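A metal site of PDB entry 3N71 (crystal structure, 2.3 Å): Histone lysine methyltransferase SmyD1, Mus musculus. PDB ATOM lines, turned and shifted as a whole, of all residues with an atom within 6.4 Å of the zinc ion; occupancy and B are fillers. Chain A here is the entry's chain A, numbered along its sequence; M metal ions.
SG of Cys 68 sits close to N of Ala 71 (3.5 Å). SG of Cys 68 sits close to N of Phe 70, at 3.5 Å. OE2 of Glu 89 is in hydrogen-bond range of ND1 of His 86. The side-chain sulfur (SG) of Cys 65 lies close to the backbone NH (N) of Gln 67, at 3.8 Å. N of Cys 65 is in hydrogen-bond range of O of Ala 71 (3.0 Å).
The nearest printed residue that does not touch the zinc ion is Gln 67 (4.3 Å).
The zinc ion is bound by the side-chain sulfur of Cys 68 (2.3 Å), a ring nitrogen (NE2) of His 86 (2.4 Å), the side-chain sulfur of Cys 90 (2.5 Å) and the side-chain sulfur of Cys 65 (2.7 Å). The zinc ion has four donor atoms within binding distance.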
ATOM      1  N   CYS A  65     -10.310  21.485  14.810  1.00  0.00           N
ATOM      2  CA  CYS A  65     -10.387  20.177  14.156  1.00  0.00           C
ATOM      3  C   CYS A  65     -10.122  20.396  12.679  1.00  0.00           C
ATOM      4  O   CYS A  65     -10.919  21.037  11.983  1.00  0.00           O
ATOM      5  CB  CYS A  65     -11.783  19.571  14.359  1.00  0.00           C
ATOM      6  SG  CYS A  65     -12.058  17.949  13.571  1.00  0.00           S
ATOM      7  N   GLY A  66      -8.999  19.874  12.192  1.00  0.00           N
ATOM      8  CA  GLY A  66      -8.657  20.037  10.791  1.00  0.00           C
ATOM      9  C   GLY A  66      -9.771  19.726   9.806  1.00  0.00           C
ATOM     10  O   GLY A  66      -9.842  20.341   8.748  1.00  0.00           O
ATOM     11  N   GLN A  67     -10.641  18.784  10.164  1.00  0.00           N
ATOM     12  CA  GLN A  67     -11.730  18.374   9.270  1.00  0.00           C
ATOM     13  C   GLN A  67     -12.950  19.295   9.132  1.00  0.00           C
ATOM     14  O   GLN A  67     -13.560  19.331   8.061  1.00  0.00           O
ATOM     15  CB  GLN A  67     -12.224  16.967   9.647  1.00  0.00           C
ATOM     16  CG  GLN A  67     -11.327  15.843   9.144  1.00  0.00           C
ATOM     17  CD  GLN A  67     -11.335  15.722   7.638  1.00  0.00           C
ATOM     18  OE1 GLN A  67     -12.374  15.445   7.033  1.00  0.00           O
ATOM     19  NE2 GLN A  67     -10.176  15.950   7.013  1.00  0.00           N
ATOM     20  N   CYS A  68     -13.297  20.042  10.179  1.00  0.00           N
ATOM     21  CA  CYS A  68     -14.479  20.914  10.085  1.00  0.00           C
ATOM     22  C   CYS A  68     -14.238  22.410  10.354  1.00  0.00           C
ATOM     23  O   CYS A  68     -15.096  23.241  10.027  1.00  0.00           O
ATOM     24  CB  CYS A  68     -15.568  20.408  11.029  1.00  0.00           C
ATOM     25  SG  CYS A  68     -15.162  20.554  12.785  1.00  0.00           S
ATOM     26  N   LYS A  69     -13.092  22.745  10.959  1.00  0.00           N
ATOM     27  CA  LYS A  69     -12.770  24.144  11.254  1.00  0.00           C
ATOM     28  C   LYS A  69     -13.793  24.788  12.188  1.00  0.00           C
ATOM     29  O   LYS A  69     -13.894  26.016  12.264  1.00  0.00           O
ATOM     30  CB  LYS A  69     -12.715  24.971   9.968  1.00  0.00           C
ATOM     31  CG  LYS A  69     -11.570  24.635   9.020  1.00  0.00           C
ATOM     32  CD  LYS A  69     -11.528  25.631   7.861  1.00  0.00           C
ATOM     33  CE  LYS A  69     -10.375  25.391   6.906  1.00  0.00           C
ATOM     34  NZ  LYS A  69     -10.349  26.437   5.841  1.00  0.00           N
ATOM     35  N   PHE A  70     -14.556  23.949  12.884  1.00  0.00           N
ATOM     36  CA  PHE A  70     -15.593  24.393  13.825  1.00  0.00           C
ATOM     37  C   PHE A  70     -15.244  24.032  15.280  1.00  0.00           C
ATOM     38  O   PHE A  70     -15.131  24.894  16.143  1.00  0.00           O
ATOM     39  CB  PHE A  70     -16.936  23.757  13.443  1.00  0.00           C
ATOM     40  CG  PHE A  70     -17.978  23.800  14.536  1.00  0.00           C
ATOM     41  CD1 PHE A  70     -18.509  25.007  14.973  1.00  0.00           C
ATOM     42  CD2 PHE A  70     -18.436  22.617  15.104  1.00  0.00           C
ATOM     43  CE1 PHE A  70     -19.492  25.042  15.960  1.00  0.00           C
ATOM     44  CE2 PHE A  70     -19.419  22.644  16.086  1.00  0.00           C
ATOM     45  CZ  PHE A  70     -19.952  23.864  16.520  1.00  0.00           C
ATOM     46  N   ALA A  71     -15.059  22.751  15.531  1.00  0.00           N
ATOM     47  CA  ALA A  71     -14.743  22.291  16.879  1.00  0.00           C
ATOM     48  C   ALA A  71     -13.357  22.735  17.292  1.00  0.00           C
ATOM     49  O   ALA A  71     -12.423  22.707  16.493  1.00  0.00           O
ATOM     50  CB  ALA A  71     -14.840  20.772  16.947  1.00  0.00           C
ATOM     51  N   TYR A  73     -10.471  22.594  20.709  1.00  0.00           N
ATOM     52  CA  TYR A  73     -10.180  21.870  21.934  1.00  0.00           C
ATOM     53  C   TYR A  73      -8.946  22.377  22.660  1.00  0.00           C
ATOM     54  O   TYR A  73      -8.128  23.112  22.101  1.00  0.00           O
ATOM     55  CB  TYR A  73     -10.003  20.394  21.606  1.00  0.00           C
ATOM     56  CG  TYR A  73     -11.142  19.795  20.798  1.00  0.00           C
ATOM     57  CD1 TYR A  73     -12.371  19.503  21.395  1.00  0.00           C
ATOM     58  CD2 TYR A  73     -10.994  19.533  19.436  1.00  0.00           C
ATOM     59  CE1 TYR A  73     -13.419  18.943  20.640  1.00  0.00           C
ATOM     60  CE2 TYR A  73     -12.019  18.978  18.690  1.00  0.00           C
ATOM     61  CZ  TYR A  73     -13.227  18.684  19.291  1.00  0.00           C
ATOM     62  OH  TYR A  73     -14.248  18.149  18.531  1.00  0.00           O
ATOM     63  N   TRP A  83     -14.679  13.012  20.275  1.00  0.00           N
ATOM     64  CA  TRP A  83     -14.954  12.267  19.052  1.00  0.00           C
ATOM     65  C   TRP A  83     -16.304  11.545  19.076  1.00  0.00           C
ATOM     66  O   TRP A  83     -17.081  11.678  18.138  1.00  0.00           O
ATOM     67  CB  TRP A  83     -13.822  11.273  18.779  1.00  0.00           C
ATOM     68  CG  TRP A  83     -13.911  10.668  17.411  1.00  0.00           C
ATOM     69  CD1 TRP A  83     -14.012   9.334  17.121  1.00  0.00           C
ATOM     70  CD2 TRP A  83     -13.954  11.359  16.161  1.00  0.00           C
ATOM     71  NE1 TRP A  83     -14.134   9.162  15.765  1.00  0.00           N
ATOM     72  CE2 TRP A  83     -14.098  10.387  15.148  1.00  0.00           C
ATOM     73  CE3 TRP A  83     -13.896  12.716  15.795  1.00  0.00           C
ATOM     74  CZ2 TRP A  83     -14.183  10.717  13.785  1.00  0.00           C
ATOM     75  CZ3 TRP A  83     -13.979  13.041  14.440  1.00  0.00           C
ATOM     76  CH2 TRP A  83     -14.124  12.053  13.454  1.00  0.00           C
ATOM     77  N   HIS A  86     -18.786  14.083  18.476  1.00  0.00           N
ATOM     78  CA  HIS A  86     -18.424  14.953  17.372  1.00  0.00           C
ATOM     79  C   HIS A  86     -18.319  14.309  15.970  1.00  0.00           C
ATOM     80  O   HIS A  86     -18.441  15.009  14.965  1.00  0.00           O
ATOM     81  CB  HIS A  86     -17.128  15.662  17.729  1.00  0.00           C
ATOM     82  CG  HIS A  86     -16.637  16.584  16.674  1.00  0.00           C
ATOM     83  ND1 HIS A  86     -17.343  17.699  16.273  1.00  0.00           N
ATOM     84  CD2 HIS A  86     -15.509  16.565  15.915  1.00  0.00           C
ATOM     85  CE1 HIS A  86     -16.667  18.323  15.311  1.00  0.00           C
ATOM     86  NE2 HIS A  86     -15.555  17.648  15.087  1.00  0.00           N
ATOM     87  N   GLU A  89     -21.560  15.181  13.868  1.00  0.00           N
ATOM     88  CA  GLU A  89     -21.766  16.593  13.509  1.00  0.00           C
ATOM     89  C   GLU A  89     -20.613  17.099  12.665  1.00  0.00           C
ATOM     90  O   GLU A  89     -20.796  18.015  11.865  1.00  0.00           O
ATOM     91  CB  GLU A  89     -21.975  17.495  14.747  1.00  0.00           C
ATOM     92  CG  GLU A  89     -20.812  17.569  15.722  1.00  0.00           C
ATOM     93  CD  GLU A  89     -20.837  18.812  16.609  1.00  0.00           C
ATOM     94  OE1 GLU A  89     -21.891  19.129  17.231  1.00  0.00           O
ATOM     95  OE2 GLU A  89     -19.795  19.481  16.698  1.00  0.00           O
ATOM     96  N   CYS A  90     -19.428  16.523  12.846  1.00  0.00           N
ATOM     97  CA  CYS A  90     -18.270  16.948  12.062  1.00  0.00           C
ATOM     98  C   CYS A  90     -18.626  16.658  10.613  1.00  0.00           C
ATOM     99  O   CYS A  90     -18.735  17.571   9.777  1.00  0.00           O
ATOM    100  CB  CYS A  90     -17.040  16.140  12.442  1.00  0.00           C
ATOM    101  SG  CYS A  90     -15.560  16.543  11.472  1.00  0.00           S
ATOM    102  N   ALA A  91     -18.815  15.376  10.333  1.00  0.00           N
ATOM    103  CA  ALA A  91     -19.164  14.907   8.994  1.00  0.00           C
ATOM    104  C   ALA A  91     -20.425  15.584   8.499  1.00  0.00           C
ATOM    105  O   ALA A  91     -20.592  15.797   7.297  1.00  0.00           O
ATOM    106  CB  ALA A  91     -19.344  13.391   9.018  1.00  0.00           C
HETATM  107 ZN    ZN M   1     -14.632  18.326  13.012  1.00  0.00          ZN
